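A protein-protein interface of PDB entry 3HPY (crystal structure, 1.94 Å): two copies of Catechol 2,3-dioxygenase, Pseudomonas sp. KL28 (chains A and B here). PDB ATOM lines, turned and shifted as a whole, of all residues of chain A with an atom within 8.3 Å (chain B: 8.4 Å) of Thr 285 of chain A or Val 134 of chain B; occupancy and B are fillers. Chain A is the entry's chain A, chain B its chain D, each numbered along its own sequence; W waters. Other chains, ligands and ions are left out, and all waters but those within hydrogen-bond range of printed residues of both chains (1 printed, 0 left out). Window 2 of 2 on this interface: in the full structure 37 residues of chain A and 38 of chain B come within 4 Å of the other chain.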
ATOM      1  N   GLU A 179     -14.759 -31.868  14.027  1.00  0.00           N
ATOM      2  CA  GLU A 179     -15.685 -31.267  14.983  1.00  0.00           C
ATOM      3  C   GLU A 179     -15.470 -29.754  15.038  1.00  0.00           C
ATOM      4  O   GLU A 179     -14.385 -29.269  14.711  1.00  0.00           O
ATOM      5  CB  GLU A 179     -15.507 -31.892  16.380  1.00  0.00           C
ATOM      6  CG  GLU A 179     -15.909 -33.368  16.441  1.00  0.00           C
ATOM      7  CD  GLU A 179     -16.587 -33.758  17.752  1.00  0.00           C
ATOM      8  OE1 GLU A 179     -17.406 -32.949  18.246  1.00  0.00           O
ATOM      9  OE2 GLU A 179     -16.319 -34.870  18.272  1.00  0.00           O
ATOM     10  N   ARG A 180     -16.511 -29.013  15.419  1.00  0.00           N
ATOM     11  CA  ARG A 180     -16.411 -27.560  15.532  1.00  0.00           C
ATOM     12  C   ARG A 180     -17.186 -27.050  16.747  1.00  0.00           C
ATOM     13  O   ARG A 180     -18.083 -27.726  17.251  1.00  0.00           O
ATOM     14  CB  ARG A 180     -16.911 -26.857  14.239  1.00  0.00           C
ATOM     15  CG  ARG A 180     -18.445 -26.833  13.963  1.00  0.00           C
ATOM     16  CD  ARG A 180     -18.817 -25.895  12.769  1.00  0.00           C
ATOM     17  NE  ARG A 180     -18.971 -26.570  11.475  1.00  0.00           N
ATOM     18  CZ  ARG A 180     -19.126 -25.948  10.304  1.00  0.00           C
ATOM     19  NH1 ARG A 180     -19.149 -24.623  10.246  1.00  0.00           N
ATOM     20  NH2 ARG A 180     -19.268 -26.651   9.183  1.00  0.00           N
ATOM     21  N   VAL A 181     -16.801 -25.872  17.231  1.00  0.00           N
ATOM     22  CA  VAL A 181     -17.460 -25.227  18.360  1.00  0.00           C
ATOM     23  C   VAL A 181     -17.996 -23.906  17.846  1.00  0.00           C
ATOM     24  O   VAL A 181     -17.227 -23.004  17.519  1.00  0.00           O
ATOM     25  CB  VAL A 181     -16.486 -24.913  19.503  1.00  0.00           C
ATOM     26  CG1 VAL A 181     -17.182 -24.062  20.557  1.00  0.00           C
ATOM     27  CG2 VAL A 181     -15.979 -26.202  20.119  1.00  0.00           C
ATOM     28  N   LEU A 182     -19.315 -23.804  17.757  1.00  0.00           N
ATOM     29  CA  LEU A 182     -19.955 -22.591  17.275  1.00  0.00           C
ATOM     30  C   LEU A 182     -19.572 -21.390  18.107  1.00  0.00           C
ATOM     31  O   LEU A 182     -19.183 -21.510  19.272  1.00  0.00           O
ATOM     32  CB  LEU A 182     -21.480 -22.736  17.306  1.00  0.00           C
ATOM     33  CG  LEU A 182     -22.163 -23.479  16.163  1.00  0.00           C
ATOM     34  CD1 LEU A 182     -21.398 -24.731  15.825  1.00  0.00           C
ATOM     35  CD2 LEU A 182     -23.593 -23.810  16.564  1.00  0.00           C
ATOM     36  N   SER A 183     -19.664 -20.222  17.490  1.00  0.00           N
ATOM     37  CA  SER A 183     -19.376 -19.013  18.217  1.00  0.00           C
ATOM     38  C   SER A 183     -20.735 -18.653  18.810  1.00  0.00           C
ATOM     39  O   SER A 183     -21.782 -19.025  18.269  1.00  0.00           O
ATOM     40  CB  SER A 183     -18.830 -17.907  17.287  1.00  0.00           C
ATOM     41  OG  SER A 183     -19.815 -17.347  16.441  1.00  0.00           O
ATOM     42  N   PRO A 184     -20.723 -17.949  19.946  1.00  0.00           N
ATOM     43  CA  PRO A 184     -21.826 -17.447  20.776  1.00  0.00           C
ATOM     44  C   PRO A 184     -23.095 -17.260  19.898  1.00  0.00           C
ATOM     45  O   PRO A 184     -24.095 -17.893  20.181  1.00  0.00           O
ATOM     46  CB  PRO A 184     -21.191 -16.226  21.432  1.00  0.00           C
ATOM     47  CG  PRO A 184     -19.728 -16.754  21.650  1.00  0.00           C
ATOM     48  CD  PRO A 184     -19.439 -17.325  20.315  1.00  0.00           C
ATOM     49  N   ASP A 187     -22.004 -16.746  15.004  1.00  0.00           N
ATOM     50  CA  ASP A 187     -21.836 -17.926  14.209  1.00  0.00           C
ATOM     51  C   ASP A 187     -20.743 -17.973  13.181  1.00  0.00           C
ATOM     52  O   ASP A 187     -20.898 -17.666  12.000  1.00  0.00           O
ATOM     53  CB  ASP A 187     -23.158 -18.347  13.613  1.00  0.00           C
ATOM     54  CG  ASP A 187     -23.755 -19.470  14.389  1.00  0.00           C
ATOM     55  OD1 ASP A 187     -23.971 -19.289  15.609  1.00  0.00           O
ATOM     56  OD2 ASP A 187     -23.970 -20.540  13.793  1.00  0.00           O
ATOM     57  N   MET A 190     -15.440 -20.958  16.864  1.00  0.00           N
ATOM     58  CA  MET A 190     -14.497 -20.475  17.852  1.00  0.00           C
ATOM     59  C   MET A 190     -13.437 -21.554  18.027  1.00  0.00           C
ATOM     60  O   MET A 190     -12.371 -21.309  18.593  1.00  0.00           O
ATOM     61  CB  MET A 190     -15.194 -20.180  19.183  1.00  0.00           C
ATOM     62  CG  MET A 190     -16.082 -18.950  19.137  1.00  0.00           C
ATOM     63  SD  MET A 190     -15.167 -17.414  18.773  1.00  0.00           S
ATOM     64  CE  MET A 190     -15.538 -16.430  20.250  1.00  0.00           C
ATOM     65  N   VAL A 250     -16.231 -33.220  23.258  1.00  0.00           N
ATOM     66  CA  VAL A 250     -15.996 -32.589  21.960  1.00  0.00           C
ATOM     67  C   VAL A 250     -15.055 -33.438  21.118  1.00  0.00           C
ATOM     68  O   VAL A 250     -14.500 -32.958  20.130  1.00  0.00           O
ATOM     69  CB  VAL A 250     -15.357 -31.188  22.096  1.00  0.00           C
ATOM     70  CG1 VAL A 250     -16.332 -30.216  22.723  1.00  0.00           C
ATOM     71  CG2 VAL A 250     -14.128 -31.278  22.942  1.00  0.00           C
ATOM     72  N   PRO A 281     -18.904 -32.854   9.710  1.00  0.00           N
ATOM     73  CA  PRO A 281     -18.422 -32.548  11.059  1.00  0.00           C
ATOM     74  C   PRO A 281     -19.499 -32.482  12.131  1.00  0.00           C
ATOM     75  O   PRO A 281     -20.665 -32.226  11.846  1.00  0.00           O
ATOM     76  CB  PRO A 281     -17.718 -31.205  10.875  1.00  0.00           C
ATOM     77  CG  PRO A 281     -18.502 -30.569   9.764  1.00  0.00           C
ATOM     78  CD  PRO A 281     -18.655 -31.725   8.798  1.00  0.00           C
ATOM     79  N   LEU A 282     -19.101 -32.743  13.369  1.00  0.00           N
ATOM     80  CA  LEU A 282     -20.031 -32.652  14.482  1.00  0.00           C
ATOM     81  C   LEU A 282     -19.853 -31.220  14.951  1.00  0.00           C
ATOM     82  O   LEU A 282     -18.824 -30.609  14.673  1.00  0.00           O
ATOM     83  CB  LEU A 282     -19.642 -33.625  15.590  1.00  0.00           C
ATOM     84  CG  LEU A 282     -19.630 -35.082  15.135  1.00  0.00           C
ATOM     85  CD1 LEU A 282     -19.413 -35.989  16.343  1.00  0.00           C
ATOM     86  CD2 LEU A 282     -20.941 -35.414  14.444  1.00  0.00           C
ATOM     87  N   SER A 283     -20.839 -30.674  15.642  1.00  0.00           N
ATOM     88  CA  SER A 283     -20.713 -29.303  16.097  1.00  0.00           C
ATOM     89  C   SER A 283     -21.123 -29.168  17.558  1.00  0.00           C
ATOM     90  O   SER A 283     -21.888 -29.983  18.082  1.00  0.00           O
ATOM     91  CB  SER A 283     -21.573 -28.381  15.221  1.00  0.00           C
ATOM     92  OG  SER A 283     -22.922 -28.427  15.637  1.00  0.00           O
ATOM     93  N   TRP A 284     -20.590 -28.139  18.210  1.00  0.00           N
ATOM     94  CA  TRP A 284     -20.894 -27.861  19.610  1.00  0.00           C
ATOM     95  C   TRP A 284     -21.307 -26.402  19.772  1.00  0.00           C
ATOM     96  O   TRP A 284     -20.700 -25.515  19.177  1.00  0.00           O
ATOM     97  CB  TRP A 284     -19.676 -28.143  20.494  1.00  0.00           C
ATOM     98  CG  TRP A 284     -19.333 -29.611  20.598  1.00  0.00           C
ATOM     99  CD1 TRP A 284     -18.549 -30.335  19.741  1.00  0.00           C
ATOM    100  CD2 TRP A 284     -19.840 -30.544  21.583  1.00  0.00           C
ATOM    101  NE1 TRP A 284     -18.542 -31.666  20.137  1.00  0.00           N
ATOM    102  CE2 TRP A 284     -19.322 -31.824  21.255  1.00  0.00           C
ATOM    103  CE3 TRP A 284     -20.679 -30.425  22.703  1.00  0.00           C
ATOM    104  CZ2 TRP A 284     -19.618 -32.988  22.015  1.00  0.00           C
ATOM    105  CZ3 TRP A 284     -20.982 -31.584  23.470  1.00  0.00           C
ATOM    106  CH2 TRP A 284     -20.443 -32.857  23.109  1.00  0.00           C
ATOM    107  N   THR A 285     -22.353 -26.153  20.555  1.00  0.00           N
ATOM    108  CA  THR A 285     -22.800 -24.783  20.794  1.00  0.00           C
ATOM    109  C   THR A 285     -21.843 -24.171  21.805  1.00  0.00           C
ATOM    110  O   THR A 285     -21.360 -24.862  22.709  1.00  0.00           O
ATOM    111  CB  THR A 285     -24.244 -24.738  21.348  1.00  0.00           C
ATOM    112  OG1 THR A 285     -24.318 -25.471  22.576  1.00  0.00           O
ATOM    113  CG2 THR A 285     -25.216 -25.345  20.349  1.00  0.00           C
ATOM    114  N   TYR A 286     -21.559 -22.883  21.647  1.00  0.00           N
ATOM    115  CA  TYR A 286     -20.638 -22.183  22.535  1.00  0.00           C
ATOM    116  C   TYR A 286     -20.903 -22.429  24.022  1.00  0.00           C
ATOM    117  O   TYR A 286     -20.011 -22.828  24.765  1.00  0.00           O
ATOM    118  CB  TYR A 286     -20.698 -20.681  22.261  1.00  0.00           C
ATOM    119  CG  TYR A 286     -19.701 -19.871  23.058  1.00  0.00           C
ATOM    120  CD1 TYR A 286     -18.350 -19.854  22.711  1.00  0.00           C
ATOM    121  CD2 TYR A 286     -20.106 -19.123  24.165  1.00  0.00           C
ATOM    122  CE1 TYR A 286     -17.425 -19.107  23.447  1.00  0.00           C
ATOM    123  CE2 TYR A 286     -19.190 -18.375  24.905  1.00  0.00           C
ATOM    124  CZ  TYR A 286     -17.855 -18.372  24.541  1.00  0.00           C
ATOM    125  OH  TYR A 286     -16.949 -17.635  25.272  1.00  0.00           O
ATOM    126  N   ASP A 287     -22.130 -22.172  24.453  1.00  0.00           N
ATOM    127  CA  ASP A 287     -22.504 -22.346  25.849  1.00  0.00           C
ATOM    128  C   ASP A 287     -22.284 -23.767  26.340  1.00  0.00           C
ATOM    129  O   ASP A 287     -21.839 -23.983  27.470  1.00  0.00           O
ATOM    130  CB  ASP A 287     -23.967 -21.962  26.037  1.00  0.00           C
ATOM    131  CG  ASP A 287     -24.804 -22.313  24.841  1.00  0.00           C
ATOM    132  OD1 ASP A 287     -24.825 -23.504  24.450  1.00  0.00           O
ATOM    133  OD2 ASP A 287     -25.435 -21.390  24.285  1.00  0.00           O
ATOM    134  N   ASN A 288     -22.595 -24.734  25.487  1.00  0.00           N
ATOM    135  CA  ASN A 288     -22.436 -26.132  25.846  1.00  0.00           C
ATOM    136  C   ASN A 288     -20.960 -26.490  25.874  1.00  0.00           C
ATOM    137  O   ASN A 288     -20.564 -27.489  26.467  1.00  0.00           O
ATOM    138  CB  ASN A 288     -23.183 -27.018  24.844  1.00  0.00           C
ATOM    139  CG  ASN A 288     -23.198 -28.478  25.251  1.00  0.00           C
ATOM    140  OD1 ASN A 288     -22.191 -29.174  25.143  1.00  0.00           O
ATOM    141  ND2 ASN A 288     -24.345 -28.947  25.729  1.00  0.00           N
ATOM    142  N   PHE A 289     -20.144 -25.657  25.245  1.00  0.00           N
ATOM    143  CA  PHE A 289     -18.709 -25.897  25.197  1.00  0.00           C
ATOM    144  C   PHE A 289     -18.058 -25.550  26.535  1.00  0.00           C
ATOM    145  O   PHE A 289     -17.209 -24.626  26.562  1.00  0.00           O
ATOM    146  CB  PHE A 289     -18.095 -25.073  24.059  1.00  0.00           C
ATOM    147  CG  PHE A 289     -16.642 -25.366  23.802  1.00  0.00           C
ATOM    148  CD1 PHE A 289     -16.196 -26.674  23.629  1.00  0.00           C
ATOM    149  CD2 PHE A 289     -15.721 -24.327  23.711  1.00  0.00           C
ATOM    150  CE1 PHE A 289     -14.849 -26.943  23.367  1.00  0.00           C
ATOM    151  CE2 PHE A 289     -14.375 -24.582  23.450  1.00  0.00           C
ATOM    152  CZ  PHE A 289     -13.939 -25.894  23.278  1.00  0.00           C
ATOM    153  N   ILE B 131     -27.322 -40.558  17.042  1.00  0.00           N
ATOM    154  CA  ILE B 131     -26.978 -39.494  17.981  1.00  0.00           C
ATOM    155  C   ILE B 131     -27.038 -38.138  17.277  1.00  0.00           C
ATOM    156  O   ILE B 131     -26.768 -38.051  16.084  1.00  0.00           O
ATOM    157  CB  ILE B 131     -25.559 -39.715  18.520  1.00  0.00           C
ATOM    158  CG1 ILE B 131     -25.479 -41.087  19.194  1.00  0.00           C
ATOM    159  CG2 ILE B 131     -25.192 -38.609  19.497  1.00  0.00           C
ATOM    160  CD1 ILE B 131     -24.077 -41.475  19.644  1.00  0.00           C
ATOM    161  N   SER B 132     -27.381 -37.079  18.003  1.00  0.00           N
ATOM    162  CA  SER B 132     -27.458 -35.753  17.396  1.00  0.00           C
ATOM    163  C   SER B 132     -26.131 -35.307  16.768  1.00  0.00           C
ATOM    164  O   SER B 132     -25.069 -35.828  17.099  1.00  0.00           O
ATOM    165  CB  SER B 132     -27.897 -34.722  18.433  1.00  0.00           C
ATOM    166  OG  SER B 132     -27.713 -33.419  17.919  1.00  0.00           O
ATOM    167  N   GLU B 133     -26.192 -34.339  15.862  1.00  0.00           N
ATOM    168  CA  GLU B 133     -24.987 -33.837  15.201  1.00  0.00           C
ATOM    169  C   GLU B 133     -24.487 -32.605  15.930  1.00  0.00           C
ATOM    170  O   GLU B 133     -23.430 -32.059  15.601  1.00  0.00           O
ATOM    171  CB  GLU B 133     -25.303 -33.465  13.757  1.00  0.00           C
ATOM    172  CG  GLU B 133     -26.332 -34.397  13.156  1.00  0.00           C
ATOM    173  CD  GLU B 133     -26.649 -34.087  11.720  1.00  0.00           C
ATOM    174  OE1 GLU B 133     -26.826 -32.894  11.393  1.00  0.00           O
ATOM    175  OE2 GLU B 133     -26.735 -35.048  10.923  1.00  0.00           O
ATOM    176  N   VAL B 134     -25.269 -32.165  16.906  1.00  0.00           N
ATOM    177  CA  VAL B 134     -24.937 -30.991  17.701  1.00  0.00           C
ATOM    178  C   VAL B 134     -24.919 -31.406  19.152  1.00  0.00           C
ATOM    179  O   VAL B 134     -25.900 -31.944  19.647  1.00  0.00           O
ATOM    180  CB  VAL B 134     -25.983 -29.885  17.520  1.00  0.00           C
ATOM    181  CG1 VAL B 134     -25.583 -28.666  18.324  1.00  0.00           C
ATOM    182  CG2 VAL B 134     -26.114 -29.533  16.040  1.00  0.00           C
ATOM    183  N   ASN B 135     -23.807 -31.141  19.831  1.00  0.00           N
ATOM    184  CA  ASN B 135     -23.650 -31.520  21.236  1.00  0.00           C
ATOM    185  C   ASN B 135     -23.972 -32.998  21.389  1.00  0.00           C
ATOM    186  O   ASN B 135     -24.762 -33.382  22.250  1.00  0.00           O
ATOM    187  CB  ASN B 135     -24.585 -30.715  22.142  1.00  0.00           C
ATOM    188  CG  ASN B 135     -24.413 -29.218  21.989  1.00  0.00           C
ATOM    189  OD1 ASN B 135     -23.301 -28.718  21.861  1.00  0.00           O
ATOM    190  ND2 ASN B 135     -25.524 -28.490  22.020  1.00  0.00           N
ATOM    191  N   PRO B 136     -23.363 -33.853  20.552  1.00  0.00           N
ATOM    192  CA  PRO B 136     -23.602 -35.298  20.605  1.00  0.00           C
ATOM    193  C   PRO B 136     -23.064 -35.972  21.859  1.00  0.00           C
ATOM    194  O   PRO B 136     -22.024 -35.581  22.390  1.00  0.00           O
ATOM    195  CB  PRO B 136     -22.898 -35.802  19.349  1.00  0.00           C
ATOM    196  CG  PRO B 136     -21.730 -34.878  19.243  1.00  0.00           C
ATOM    197  CD  PRO B 136     -22.366 -33.531  19.511  1.00  0.00           C
ATOM    198  N   ALA B 137     -23.774 -36.987  22.336  1.00  0.00           N
ATOM    199  CA  ALA B 137     -23.308 -37.722  23.502  1.00  0.00           C
ATOM    200  C   ALA B 137     -22.273 -38.729  22.989  1.00  0.00           C
ATOM    201  O   ALA B 137     -22.152 -38.950  21.777  1.00  0.00           O
ATOM    202  CB  ALA B 137     -24.461 -38.438  24.170  1.00  0.00           C
HETATM  203  O   HOH W   1     -22.737 -30.552  12.758  1.00  0.00           O
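O of Glu 133 of chain B is in hydrogen-bond range of N of Ser 283 of chain A, 2.9 Å away.
The backbone NH (N) of Asn 135 of chain B is in hydrogen-bond range of the backbone carbonyl oxygen (O) of Ser 283 of chain A, 2.8 Å away.
N of Thr 285 of chain A lies within hydrogen-bond range of OD1 of Asn 135 of chain B (3.0 Å).
The side-chain amide oxygen (OD1) of Asn 135 of chain B lies close to the side-chain amide oxygen (OD1) of Asn 288 of chain A (3.5 Å).
NE1 of Trp 284 of chain A is in hydrogen-bond range of OE1 of Glu 179 of chain A (2.6 Å).
N of Arg 180 of chain A lies within hydrogen-bond range of O of Leu 282 of chain A (2.9 Å).
The backbone carbonyl oxygen (O) of Arg 180 of chain A lies within hydrogen-bond range of the backbone NH (N) of Trp 284 of chain A (2.7 Å).
The side-chain hydroxyl (OG1) of Thr 285 of chain A sits at hydrogen-bond distance from the side-chain carboxylate (OD1) of Asp 287 of chain A, at 2.8 Å.
N of Asn 288 of chain A sits close to OG1 of Thr 285 of chain A (3.5 Å).
The side-chain hydroxyl of Ser 132 of chain B lies within hydrogen-bond range of the backbone carbonyl oxygen of Val 134 of chain B (2.9 Å).
Among the printed residues, merely in contact across the chains: Leu 282 of chain A with Glu 133 of chain B, Leu 282 of chain A with Pro 136 of chain B, Ser 283 of chain A with Val 134 of chain B, Ser 283 of chain A with Pro 136 of chain B, Trp 284 of chain A with Asn 135 of chain B, Trp 284 of chain A with Pro 136 of chain B and Thr 285 of chain A with Val 134 of chain B.
Thr 285 of chain A touches two residues of chain B.
Val 134 of chain B touches just these residues of chain A: Ser 283 (3.2 Å) and Thr 285 (3.9 Å).
Of the printed residues of chain A, Pro 136 of chain B touches Leu 282 (3.9 Å), Ser 283 (3.9 Å) and Trp 284 (3.2 Å).
Printed residues of chain B within 4 Å of Asn 288 of chain A: Asn 135 (3.4 Å).
Met 190 of chain A touches none of the printed residues of chain B.
The nearest residue of chain A that does not touch Val 134 of chain B is Trp 284 of chain A (4.9 Å).
Hydrophobic or aromatic side chains of chain B that line the printed part of chain A: Val 134 and Pro 136.
Hydrophobic or aromatic side chains of chain A that line the printed part of chain B: Leu 282 and Trp 284.
Among the printed residues, 11 pairs touch across the chains.
Among the printed residues, no Asp or Glu carboxylate lies within 4 Å of a Lys or Arg side-chain nitrogen of the other chain.
No position is printed for both chains.
Water W1 lies within hydrogen-bond range of O of Pro 281 of chain A, O of Glu 133 of chain B and N of Ser 283 of chain A.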
